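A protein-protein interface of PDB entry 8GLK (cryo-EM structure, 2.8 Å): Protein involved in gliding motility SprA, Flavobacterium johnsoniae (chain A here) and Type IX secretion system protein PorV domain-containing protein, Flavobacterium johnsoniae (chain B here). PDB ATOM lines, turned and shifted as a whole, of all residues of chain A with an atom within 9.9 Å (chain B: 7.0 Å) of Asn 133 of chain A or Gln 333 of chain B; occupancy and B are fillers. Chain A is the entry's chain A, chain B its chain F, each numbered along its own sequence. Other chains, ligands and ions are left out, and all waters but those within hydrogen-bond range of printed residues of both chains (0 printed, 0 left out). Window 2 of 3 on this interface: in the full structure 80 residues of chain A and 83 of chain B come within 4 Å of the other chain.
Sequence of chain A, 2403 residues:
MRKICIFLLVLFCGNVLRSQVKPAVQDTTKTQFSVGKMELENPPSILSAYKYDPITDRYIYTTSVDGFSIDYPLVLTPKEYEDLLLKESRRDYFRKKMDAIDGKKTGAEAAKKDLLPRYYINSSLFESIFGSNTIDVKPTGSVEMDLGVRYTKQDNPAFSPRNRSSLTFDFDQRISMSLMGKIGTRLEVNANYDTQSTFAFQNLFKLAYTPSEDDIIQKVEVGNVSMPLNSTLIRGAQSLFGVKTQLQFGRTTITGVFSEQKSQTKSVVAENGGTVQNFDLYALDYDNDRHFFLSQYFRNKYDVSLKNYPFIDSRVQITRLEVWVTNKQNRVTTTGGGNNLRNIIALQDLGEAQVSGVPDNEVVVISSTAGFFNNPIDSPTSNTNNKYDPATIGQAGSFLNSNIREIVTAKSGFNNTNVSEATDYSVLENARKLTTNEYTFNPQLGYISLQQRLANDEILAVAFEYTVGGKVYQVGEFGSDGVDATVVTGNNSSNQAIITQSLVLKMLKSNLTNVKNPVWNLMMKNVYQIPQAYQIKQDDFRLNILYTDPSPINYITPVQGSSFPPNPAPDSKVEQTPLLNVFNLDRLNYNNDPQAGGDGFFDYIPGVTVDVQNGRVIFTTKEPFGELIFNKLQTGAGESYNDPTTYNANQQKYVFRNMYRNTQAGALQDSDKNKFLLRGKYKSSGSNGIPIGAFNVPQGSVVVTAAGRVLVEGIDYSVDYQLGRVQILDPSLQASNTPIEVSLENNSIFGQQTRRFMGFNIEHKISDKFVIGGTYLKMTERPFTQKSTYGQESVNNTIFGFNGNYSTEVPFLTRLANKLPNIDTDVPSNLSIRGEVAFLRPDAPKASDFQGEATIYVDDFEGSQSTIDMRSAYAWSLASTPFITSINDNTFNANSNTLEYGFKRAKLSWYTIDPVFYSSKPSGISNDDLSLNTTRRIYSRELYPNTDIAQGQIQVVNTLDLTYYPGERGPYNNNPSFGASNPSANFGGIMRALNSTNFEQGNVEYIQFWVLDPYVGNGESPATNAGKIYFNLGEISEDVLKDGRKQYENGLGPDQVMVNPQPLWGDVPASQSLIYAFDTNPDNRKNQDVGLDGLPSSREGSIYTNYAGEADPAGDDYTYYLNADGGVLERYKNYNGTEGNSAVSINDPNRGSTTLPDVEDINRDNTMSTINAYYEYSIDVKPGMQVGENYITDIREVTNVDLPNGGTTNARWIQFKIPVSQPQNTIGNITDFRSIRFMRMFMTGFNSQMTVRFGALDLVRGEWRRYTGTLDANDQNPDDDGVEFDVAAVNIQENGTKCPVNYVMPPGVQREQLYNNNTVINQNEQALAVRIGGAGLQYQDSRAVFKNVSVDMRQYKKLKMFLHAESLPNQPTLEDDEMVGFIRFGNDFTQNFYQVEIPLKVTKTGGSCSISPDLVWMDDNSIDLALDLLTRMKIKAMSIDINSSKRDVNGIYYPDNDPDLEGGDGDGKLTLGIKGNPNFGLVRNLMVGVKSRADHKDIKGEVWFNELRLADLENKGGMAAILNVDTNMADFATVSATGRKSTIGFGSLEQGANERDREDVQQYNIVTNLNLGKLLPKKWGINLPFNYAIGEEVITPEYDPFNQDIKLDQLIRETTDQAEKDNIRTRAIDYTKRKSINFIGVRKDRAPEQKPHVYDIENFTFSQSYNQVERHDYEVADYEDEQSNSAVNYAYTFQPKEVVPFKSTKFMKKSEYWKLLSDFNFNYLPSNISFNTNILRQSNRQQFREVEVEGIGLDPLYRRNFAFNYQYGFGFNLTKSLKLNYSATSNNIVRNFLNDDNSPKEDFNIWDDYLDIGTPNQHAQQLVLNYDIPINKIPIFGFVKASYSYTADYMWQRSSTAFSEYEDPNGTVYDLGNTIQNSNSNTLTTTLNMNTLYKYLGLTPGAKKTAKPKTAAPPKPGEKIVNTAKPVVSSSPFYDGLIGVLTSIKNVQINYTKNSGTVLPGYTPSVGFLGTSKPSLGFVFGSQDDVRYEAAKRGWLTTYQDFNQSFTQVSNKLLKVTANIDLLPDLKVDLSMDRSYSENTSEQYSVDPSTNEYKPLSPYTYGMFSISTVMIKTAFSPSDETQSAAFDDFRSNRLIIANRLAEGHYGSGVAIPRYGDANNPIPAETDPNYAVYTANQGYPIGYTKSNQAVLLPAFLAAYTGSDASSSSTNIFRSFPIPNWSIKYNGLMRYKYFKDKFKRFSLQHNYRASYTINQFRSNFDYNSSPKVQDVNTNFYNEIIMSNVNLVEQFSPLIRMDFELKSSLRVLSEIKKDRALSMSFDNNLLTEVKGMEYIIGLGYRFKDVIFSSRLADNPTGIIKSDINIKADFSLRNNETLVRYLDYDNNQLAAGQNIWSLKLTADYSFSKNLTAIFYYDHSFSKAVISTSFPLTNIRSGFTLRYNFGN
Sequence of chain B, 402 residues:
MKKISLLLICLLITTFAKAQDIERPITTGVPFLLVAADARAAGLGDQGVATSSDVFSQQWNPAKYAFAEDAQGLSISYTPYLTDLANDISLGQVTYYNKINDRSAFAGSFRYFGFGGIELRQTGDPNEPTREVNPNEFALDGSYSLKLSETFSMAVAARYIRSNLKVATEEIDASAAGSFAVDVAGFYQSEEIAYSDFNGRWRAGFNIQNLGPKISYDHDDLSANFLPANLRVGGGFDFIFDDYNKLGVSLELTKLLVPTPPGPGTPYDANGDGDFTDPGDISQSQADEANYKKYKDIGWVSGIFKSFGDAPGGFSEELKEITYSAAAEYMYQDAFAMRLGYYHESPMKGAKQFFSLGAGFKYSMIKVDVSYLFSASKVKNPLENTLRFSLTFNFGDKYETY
OG1 of Thr 134 of chain A lies within hydrogen-bond range of OG of Ser 132 of chain A.
The backbone carbonyl oxygen (O) of Gly 184 of chain A is in hydrogen-bond range of the backbone NH (N) of Ser 132 of chain A.
N of Gln 333 of chain B sits at hydrogen-bond distance from O of Tyr 244 of chain B, 3.1 Å away.
The side-chain amide oxygen (OD1) of Asn 245 of chain B is in hydrogen-bond range of the side-chain hydroxyl (OH) of Tyr 330 of chain B (2.5 Å).
The backbone carbonyl oxygen of Ala 335 of chain B sits at hydrogen-bond distance from the backbone NH of Lys 362 of chain B (3.1 Å).
The backbone carbonyl oxygen (O) of Ser 132 of chain A lies within hydrogen-bond range of the side-chain hydroxyl (OH) of Tyr 332 of chain B, at 2.7 Å.
Among the printed residues, pairs that only touch across the chains: Phe 130 of chain A with Tyr 332 of chain B, Ile 183 of chain A with Phe 336 of chain B, Phe 130 of chain A with Tyr 330 of chain B, Asn 133 of chain A with Tyr 332 of chain B, Ile 135 of chain A with Ala 335 of chain B, Ile 135 of chain A with Gln 333 of chain B, Asn 133 of chain A with Gln 333 of chain B, Ile 183 of chain A with Tyr 332 of chain B and Ile 129 of chain A with Tyr 330 of chain B.
Of the 14 printed residues of chain A, 6 touch a printed residue of chain B.
Hydrophobic or aromatic side chains of chain A that line the printed part of chain B: Ile 129, Phe 130, Ile 135 and Ile 183.
Of the 12 printed residues of chain B, 5 touch a printed residue of chain A.
Along chain B the printed residues that touch a printed residue of chain A span positions 330 to 336.
Among the printed residues, no Asp or Glu carboxylate lies within 4 Å of a Lys or Arg side-chain nitrogen of the other chain.
Of chain B, only Tyr 332 (3.6 Å) and Gln 333 (3.7 Å) come within 4 Å of Asn 133 of chain A.
Of the printed residues of chain A, Gln 333 of chain B touches Asn 133 (3.7 Å) and Ile 135 (3.6 Å).
No residue of chain A comes within 4 Å of Tyr 244 of chain B.
Printed residues of chain A within 4 Å of Tyr 332 of chain B: Phe 130 (3.4 Å), Ser 132 (2.7 Å), Asn 133 (3.6 Å) and Ile 183 (3.9 Å).
Asp 334 of chain B touches none of the printed residues of chain A.
Of the printed residues of chain B, Ile 129 of chain A touches Tyr 330 (3.97 Å).
Of the printed residues of chain B, Phe 130 of chain A touches Tyr 330 and Tyr 332.
Printed residues of chain B within 4 Å of Ile 135 of chain A: Gln 333 and Ala 335.
Printed residues of chain B within 4 Å of Ser 132 of chain A: Tyr 332.
Printed residues of chain A within 4 Å of Phe 336 of chain B: Ile 183.
The nearest residue of chain B that does not touch Asn 133 of chain A is Tyr 244 of chain B (6.2 Å).
The nearest printed residue of chain B that does not touch Ile 183 of chain A is Ala 335 of chain B (5.8 Å).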
ATOM      1  N   ILE A 129      22.687  12.537  21.653  1.00  0.00           N
ATOM      2  CA  ILE A 129      22.953  12.518  23.085  1.00  0.00           C
ATOM      3  C   ILE A 129      23.589  11.185  23.476  1.00  0.00           C
ATOM      4  O   ILE A 129      24.454  11.130  24.351  1.00  0.00           O
ATOM      5  CB  ILE A 129      21.664  12.800  23.890  1.00  0.00           C
ATOM      6  CG1 ILE A 129      21.907  12.626  25.391  1.00  0.00           C
ATOM      7  CG2 ILE A 129      20.514  11.928  23.398  1.00  0.00           C
ATOM      8  CD1 ILE A 129      20.748  13.072  26.252  1.00  0.00           C
ATOM      9  N   PHE A 130      23.170  10.112  22.808  1.00  0.00           N
ATOM     10  CA  PHE A 130      23.766   8.797  22.984  1.00  0.00           C
ATOM     11  C   PHE A 130      24.105   8.212  21.621  1.00  0.00           C
ATOM     12  O   PHE A 130      23.410   8.460  20.631  1.00  0.00           O
ATOM     13  CB  PHE A 130      22.833   7.840  23.744  1.00  0.00           C
ATOM     14  CG  PHE A 130      22.350   8.377  25.062  1.00  0.00           C
ATOM     15  CD1 PHE A 130      23.126   8.261  26.202  1.00  0.00           C
ATOM     16  CD2 PHE A 130      21.114   8.991  25.163  1.00  0.00           C
ATOM     17  CE1 PHE A 130      22.679   8.751  27.415  1.00  0.00           C
ATOM     18  CE2 PHE A 130      20.663   9.483  26.372  1.00  0.00           C
ATOM     19  CZ  PHE A 130      21.447   9.363  27.499  1.00  0.00           C
ATOM     20  N   GLY A 131      25.188   7.435  21.581  1.00  0.00           N
ATOM     21  CA  GLY A 131      25.631   6.866  20.318  1.00  0.00           C
ATOM     22  C   GLY A 131      24.659   5.852  19.749  1.00  0.00           C
ATOM     23  O   GLY A 131      24.405   5.833  18.541  1.00  0.00           O
ATOM     24  N   SER A 132      24.103   4.998  20.603  1.00  0.00           N
ATOM     25  CA  SER A 132      23.165   3.971  20.170  1.00  0.00           C
ATOM     26  C   SER A 132      22.180   3.713  21.304  1.00  0.00           C
ATOM     27  O   SER A 132      22.095   4.483  22.265  1.00  0.00           O
ATOM     28  CB  SER A 132      23.910   2.699  19.747  1.00  0.00           C
ATOM     29  OG  SER A 132      24.606   2.127  20.840  1.00  0.00           O
ATOM     30  N   ASN A 133      21.427   2.622  21.186  1.00  0.00           N
ATOM     31  CA  ASN A 133      20.466   2.223  22.204  1.00  0.00           C
ATOM     32  C   ASN A 133      20.851   0.931  22.908  1.00  0.00           C
ATOM     33  O   ASN A 133      20.071   0.429  23.723  1.00  0.00           O
ATOM     34  CB  ASN A 133      19.070   2.080  21.586  1.00  0.00           C
ATOM     35  CG  ASN A 133      19.069   1.208  20.346  1.00  0.00           C
ATOM     36  OD1 ASN A 133      19.322   1.684  19.239  1.00  0.00           O
ATOM     37  ND2 ASN A 133      18.780  -0.076  20.525  1.00  0.00           N
ATOM     38  N   THR A 134      22.026   0.379  22.616  1.00  0.00           N
ATOM     39  CA  THR A 134      22.465  -0.841  23.280  1.00  0.00           C
ATOM     40  C   THR A 134      22.819  -0.548  24.732  1.00  0.00           C
ATOM     41  O   THR A 134      23.564   0.391  25.025  1.00  0.00           O
ATOM     42  CB  THR A 134      23.669  -1.440  22.554  1.00  0.00           C
ATOM     43  OG1 THR A 134      24.721  -0.469  22.489  1.00  0.00           O
ATOM     44  CG2 THR A 134      23.286  -1.859  21.143  1.00  0.00           C
ATOM     45  N   ILE A 135      22.281  -1.356  25.642  1.00  0.00           N
ATOM     46  CA  ILE A 135      22.499  -1.200  27.077  1.00  0.00           C
ATOM     47  C   ILE A 135      22.938  -2.560  27.605  1.00  0.00           C
ATOM     48  O   ILE A 135      22.102  -3.430  27.873  1.00  0.00           O
ATOM     49  CB  ILE A 135      21.251  -0.698  27.809  1.00  0.00           C
ATOM     50  CG1 ILE A 135      20.780   0.626  27.204  1.00  0.00           C
ATOM     51  CG2 ILE A 135      21.533  -0.535  29.294  1.00  0.00           C
ATOM     52  CD1 ILE A 135      19.507   1.157  27.812  1.00  0.00           C
ATOM     53  N   ASP A 136      24.247  -2.750  27.755  1.00  0.00           N
ATOM     54  CA  ASP A 136      24.821  -4.010  28.213  1.00  0.00           C
ATOM     55  C   ASP A 136      25.426  -3.878  29.607  1.00  0.00           C
ATOM     56  O   ASP A 136      26.470  -4.459  29.907  1.00  0.00           O
ATOM     57  CB  ASP A 136      25.865  -4.520  27.222  1.00  0.00           C
ATOM     58  CG  ASP A 136      26.990  -3.529  26.994  1.00  0.00           C
ATOM     59  OD1 ASP A 136      26.859  -2.364  27.422  1.00  0.00           O
ATOM     60  OD2 ASP A 136      28.009  -3.917  26.383  1.00  0.00           O
ATOM     61  N   VAL A 137      24.774  -3.108  30.478  1.00  0.00           N
ATOM     62  CA  VAL A 137      25.221  -2.972  31.859  1.00  0.00           C
ATOM     63  C   VAL A 137      24.861  -4.245  32.608  1.00  0.00           C
ATOM     64  O   VAL A 137      23.712  -4.431  33.025  1.00  0.00           O
ATOM     65  CB  VAL A 137      24.603  -1.736  32.535  1.00  0.00           C
ATOM     66  CG1 VAL A 137      25.272  -1.476  33.873  1.00  0.00           C
ATOM     67  CG2 VAL A 137      24.728  -0.526  31.633  1.00  0.00           C
ATOM     68  N   LYS A 182      28.037  -0.669  29.498  1.00  0.00           N
ATOM     69  CA  LYS A 182      27.992   0.552  28.709  1.00  0.00           C
ATOM     70  C   LYS A 182      26.545   0.885  28.369  1.00  0.00           C
ATOM     71  O   LYS A 182      25.666   0.021  28.366  1.00  0.00           O
ATOM     72  CB  LYS A 182      28.814   0.426  27.420  1.00  0.00           C
ATOM     73  CG  LYS A 182      30.309   0.290  27.641  1.00  0.00           C
ATOM     74  CD  LYS A 182      31.049   0.154  26.322  1.00  0.00           C
ATOM     75  CE  LYS A 182      31.010   1.453  25.534  1.00  0.00           C
ATOM     76  NZ  LYS A 182      31.792   2.532  26.200  1.00  0.00           N
ATOM     77  N   ILE A 183      26.317   2.164  28.088  1.00  0.00           N
ATOM     78  CA  ILE A 183      25.010   2.688  27.709  1.00  0.00           C
ATOM     79  C   ILE A 183      25.211   3.557  26.477  1.00  0.00           C
ATOM     80  O   ILE A 183      25.849   4.617  26.555  1.00  0.00           O
ATOM     81  CB  ILE A 183      24.353   3.491  28.839  1.00  0.00           C
ATOM     82  CG1 ILE A 183      24.103   2.596  30.051  1.00  0.00           C
ATOM     83  CG2 ILE A 183      23.052   4.117  28.359  1.00  0.00           C
ATOM     84  CD1 ILE A 183      23.664   3.344  31.280  1.00  0.00           C
ATOM     85  N   GLY A 184      24.688   3.100  25.339  1.00  0.00           N
ATOM     86  CA  GLY A 184      24.720   3.877  24.111  1.00  0.00           C
ATOM     87  C   GLY A 184      26.105   4.248  23.642  1.00  0.00           C
ATOM     88  O   GLY A 184      26.296   5.351  23.120  1.00  0.00           O
ATOM     89  N   THR A 185      27.091   3.370  23.861  1.00  0.00           N
ATOM     90  CA  THR A 185      28.499   3.551  23.474  1.00  0.00           C
ATOM     91  C   THR A 185      29.048   4.914  23.901  1.00  0.00           C
ATOM     92  O   THR A 185      30.091   5.360  23.410  1.00  0.00           O
ATOM     93  CB  THR A 185      28.725   3.304  21.970  1.00  0.00           C
ATOM     94  OG1 THR A 185      30.117   3.058  21.735  1.00  0.00           O
ATOM     95  CG2 THR A 185      28.290   4.484  21.103  1.00  0.00           C
ATOM     96  N   ARG A 186      28.378   5.566  24.845  1.00  0.00           N
ATOM     97  CA  ARG A 186      28.778   6.863  25.373  1.00  0.00           C
ATOM     98  C   ARG A 186      28.983   6.852  26.876  1.00  0.00           C
ATOM     99  O   ARG A 186      29.892   7.520  27.374  1.00  0.00           O
ATOM    100  CB  ARG A 186      27.734   7.931  25.012  1.00  0.00           C
ATOM    101  CG  ARG A 186      27.685   8.286  23.537  1.00  0.00           C
ATOM    102  CD  ARG A 186      28.900   9.096  23.122  1.00  0.00           C
ATOM    103  NE  ARG A 186      28.832   9.505  21.723  1.00  0.00           N
ATOM    104  CZ  ARG A 186      28.149  10.552  21.281  1.00  0.00           C
ATOM    105  NH1 ARG A 186      27.455  11.321  22.104  1.00  0.00           N
ATOM    106  NH2 ARG A 186      28.163  10.834  19.982  1.00  0.00           N
ATOM    107  N   ASP B 243       9.154   9.198  22.752  1.00  0.00           N
ATOM    108  CA  ASP B 243       8.558   7.973  23.280  1.00  0.00           C
ATOM    109  C   ASP B 243       9.581   7.067  23.956  1.00  0.00           C
ATOM    110  O   ASP B 243       9.198   6.034  24.518  1.00  0.00           O
ATOM    111  CB  ASP B 243       7.812   7.168  22.204  1.00  0.00           C
ATOM    112  CG  ASP B 243       6.699   6.313  22.778  1.00  0.00           C
ATOM    113  OD1 ASP B 243       6.441   6.408  23.996  1.00  0.00           O
ATOM    114  OD2 ASP B 243       6.083   5.544  22.011  1.00  0.00           O
ATOM    115  N   TYR B 244      10.867   7.422  23.935  1.00  0.00           N
ATOM    116  CA  TYR B 244      11.910   6.634  24.572  1.00  0.00           C
ATOM    117  C   TYR B 244      12.648   7.399  25.661  1.00  0.00           C
ATOM    118  O   TYR B 244      13.486   6.808  26.352  1.00  0.00           O
ATOM    119  CB  TYR B 244      12.917   6.134  23.525  1.00  0.00           C
ATOM    120  CG  TYR B 244      12.478   4.889  22.786  1.00  0.00           C
ATOM    121  CD1 TYR B 244      11.266   4.276  23.074  1.00  0.00           C
ATOM    122  CD2 TYR B 244      13.282   4.319  21.808  1.00  0.00           C
ATOM    123  CE1 TYR B 244      10.863   3.136  22.404  1.00  0.00           C
ATOM    124  CE2 TYR B 244      12.887   3.179  21.132  1.00  0.00           C
ATOM    125  CZ  TYR B 244      11.677   2.594  21.434  1.00  0.00           C
ATOM    126  OH  TYR B 244      11.281   1.459  20.765  1.00  0.00           O
ATOM    127  N   ASN B 245      12.368   8.688  25.834  1.00  0.00           N
ATOM    128  CA  ASN B 245      12.988   9.500  26.870  1.00  0.00           C
ATOM    129  C   ASN B 245      11.902  10.069  27.770  1.00  0.00           C
ATOM    130  O   ASN B 245      10.848  10.490  27.285  1.00  0.00           O
ATOM    131  CB  ASN B 245      13.822  10.631  26.262  1.00  0.00           C
ATOM    132  CG  ASN B 245      14.973  10.119  25.420  1.00  0.00           C
ATOM    133  OD1 ASN B 245      16.107  10.024  25.890  1.00  0.00           O
ATOM    134  ND2 ASN B 245      14.688   9.786  24.167  1.00  0.00           N
ATOM    135  N   LYS B 246      12.159  10.081  29.074  1.00  0.00           N
ATOM    136  CA  LYS B 246      11.218  10.616  30.045  1.00  0.00           C
ATOM    137  C   LYS B 246      11.938  11.557  30.998  1.00  0.00           C
ATOM    138  O   LYS B 246      13.108  11.355  31.326  1.00  0.00           O
ATOM    139  CB  LYS B 246      10.536   9.501  30.849  1.00  0.00           C
ATOM    140  CG  LYS B 246       9.425   8.778  30.110  1.00  0.00           C
ATOM    141  CD  LYS B 246       8.923   7.593  30.916  1.00  0.00           C
ATOM    142  CE  LYS B 246       8.271   8.046  32.213  1.00  0.00           C
ATOM    143  NZ  LYS B 246       7.678   6.909  32.968  1.00  0.00           N
ATOM    144  N   TYR B 330      15.366  11.413  35.095  1.00  0.00           N
ATOM    145  CA  TYR B 330      15.473  11.231  33.656  1.00  0.00           C
ATOM    146  C   TYR B 330      15.591   9.747  33.337  1.00  0.00           C
ATOM    147  O   TYR B 330      16.458   9.054  33.882  1.00  0.00           O
ATOM    148  CB  TYR B 330      16.679  11.990  33.100  1.00  0.00           C
ATOM    149  CG  TYR B 330      16.950  11.714  31.640  1.00  0.00           C
ATOM    150  CD1 TYR B 330      16.085  12.172  30.655  1.00  0.00           C
ATOM    151  CD2 TYR B 330      18.069  10.994  31.244  1.00  0.00           C
ATOM    152  CE1 TYR B 330      16.326  11.922  29.320  1.00  0.00           C
ATOM    153  CE2 TYR B 330      18.319  10.740  29.909  1.00  0.00           C
ATOM    154  CZ  TYR B 330      17.444  11.206  28.951  1.00  0.00           C
ATOM    155  OH  TYR B 330      17.687  10.955  27.621  1.00  0.00           O
ATOM    156  N   MET B 331      14.716   9.273  32.454  1.00  0.00           N
ATOM    157  CA  MET B 331      14.645   7.879  32.040  1.00  0.00           C
ATOM    158  C   MET B 331      15.048   7.769  30.578  1.00  0.00           C
ATOM    159  O   MET B 331      14.468   8.442  29.719  1.00  0.00           O
ATOM    160  CB  MET B 331      13.230   7.326  32.226  1.00  0.00           C
ATOM    161  CG  MET B 331      12.756   7.239  33.665  1.00  0.00           C
ATOM    162  SD  MET B 331      13.776   6.149  34.667  1.00  0.00           S
ATOM    163  CE  MET B 331      13.362   4.555  33.963  1.00  0.00           C
ATOM    164  N   TYR B 332      16.030   6.917  30.298  1.00  0.00           N
ATOM    165  CA  TYR B 332      16.483   6.633  28.943  1.00  0.00           C
ATOM    166  C   TYR B 332      16.262   5.156  28.655  1.00  0.00           C
ATOM    167  O   TYR B 332      16.742   4.295  29.404  1.00  0.00           O
ATOM    168  CB  TYR B 332      17.955   7.007  28.759  1.00  0.00           C
ATOM    169  CG  TYR B 332      18.528   6.583  27.426  1.00  0.00           C
ATOM    170  CD1 TYR B 332      18.083   7.157  26.244  1.00  0.00           C
ATOM    171  CD2 TYR B 332      19.523   5.617  27.352  1.00  0.00           C
ATOM    172  CE1 TYR B 332      18.603   6.773  25.023  1.00  0.00           C
ATOM    173  CE2 TYR B 332      20.052   5.230  26.136  1.00  0.00           C
ATOM    174  CZ  TYR B 332      19.589   5.811  24.976  1.00  0.00           C
ATOM    175  OH  TYR B 332      20.111   5.429  23.761  1.00  0.00           O
ATOM    176  N   GLN B 333      15.524   4.873  27.579  1.00  0.00           N
ATOM    177  CA  GLN B 333      15.209   3.519  27.124  1.00  0.00           C
ATOM    178  C   GLN B 333      14.493   2.696  28.190  1.00  0.00           C
ATOM    179  O   GLN B 333      14.444   1.465  28.095  1.00  0.00           O
ATOM    180  CB  GLN B 333      16.470   2.783  26.656  1.00  0.00           C
ATOM    181  CG  GLN B 333      17.124   3.388  25.427  1.00  0.00           C
ATOM    182  CD  GLN B 333      16.226   3.352  24.210  1.00  0.00           C
ATOM    183  OE1 GLN B 333      15.735   4.385  23.757  1.00  0.00           O
ATOM    184  NE2 GLN B 333      16.008   2.158  23.670  1.00  0.00           N
ATOM    185  N   ASP B 334      13.930   3.357  29.204  1.00  0.00           N
ATOM    186  CA  ASP B 334      13.318   2.709  30.362  1.00  0.00           C
ATOM    187  C   ASP B 334      14.285   1.730  31.029  1.00  0.00           C
ATOM    188  O   ASP B 334      13.864   0.756  31.659  1.00  0.00           O
ATOM    189  CB  ASP B 334      12.008   2.005  29.974  1.00  0.00           C
ATOM    190  CG  ASP B 334      11.033   1.880  31.139  1.00  0.00           C
ATOM    191  OD1 ASP B 334      11.426   1.420  32.231  1.00  0.00           O
ATOM    192  OD2 ASP B 334       9.855   2.253  30.958  1.00  0.00           O
ATOM    193  N   ALA B 335      15.589   1.966  30.877  1.00  0.00           N
ATOM    194  CA  ALA B 335      16.606   1.118  31.475  1.00  0.00           C
ATOM    195  C   ALA B 335      17.735   1.890  32.137  1.00  0.00           C
ATOM    196  O   ALA B 335      18.510   1.285  32.886  1.00  0.00           O
ATOM    197  CB  ALA B 335      17.204   0.167  30.425  1.00  0.00           C
ATOM    198  N   PHE B 336      17.861   3.191  31.888  1.00  0.00           N
ATOM    199  CA  PHE B 336      18.822   4.034  32.587  1.00  0.00           C
ATOM    200  C   PHE B 336      18.073   5.168  33.268  1.00  0.00           C
ATOM    201  O   PHE B 336      17.217   5.808  32.652  1.00  0.00           O
ATOM    202  CB  PHE B 336      19.880   4.591  31.634  1.00  0.00           C
ATOM    203  CG  PHE B 336      20.822   5.564  32.283  1.00  0.00           C
ATOM    204  CD1 PHE B 336      21.588   5.184  33.372  1.00  0.00           C
ATOM    205  CD2 PHE B 336      20.940   6.858  31.807  1.00  0.00           C
ATOM    206  CE1 PHE B 336      22.453   6.075  33.973  1.00  0.00           C
ATOM    207  CE2 PHE B 336      21.804   7.754  32.404  1.00  0.00           C
ATOM    208  CZ  PHE B 336      22.561   7.361  33.488  1.00  0.00           C
ATOM    209  N   LYS B 362      18.586  -1.274  34.548  1.00  0.00           N
ATOM    210  CA  LYS B 362      17.841  -2.518  34.373  1.00  0.00           C
ATOM    211  C   LYS B 362      18.521  -3.352  33.296  1.00  0.00           C
ATOM    212  O   LYS B 362      18.597  -2.927  32.138  1.00  0.00           O
ATOM    213  CB  LYS B 362      16.387  -2.238  33.995  1.00  0.00           C
ATOM    214  CG  LYS B 362      15.548  -3.490  33.795  1.00  0.00           C
ATOM    215  CD  LYS B 362      14.152  -3.152  33.296  1.00  0.00           C
ATOM    216  CE  LYS B 362      14.187  -2.609  31.877  1.00  0.00           C
ATOM    217  NZ  LYS B 362      12.822  -2.315  31.361  1.00  0.00           N
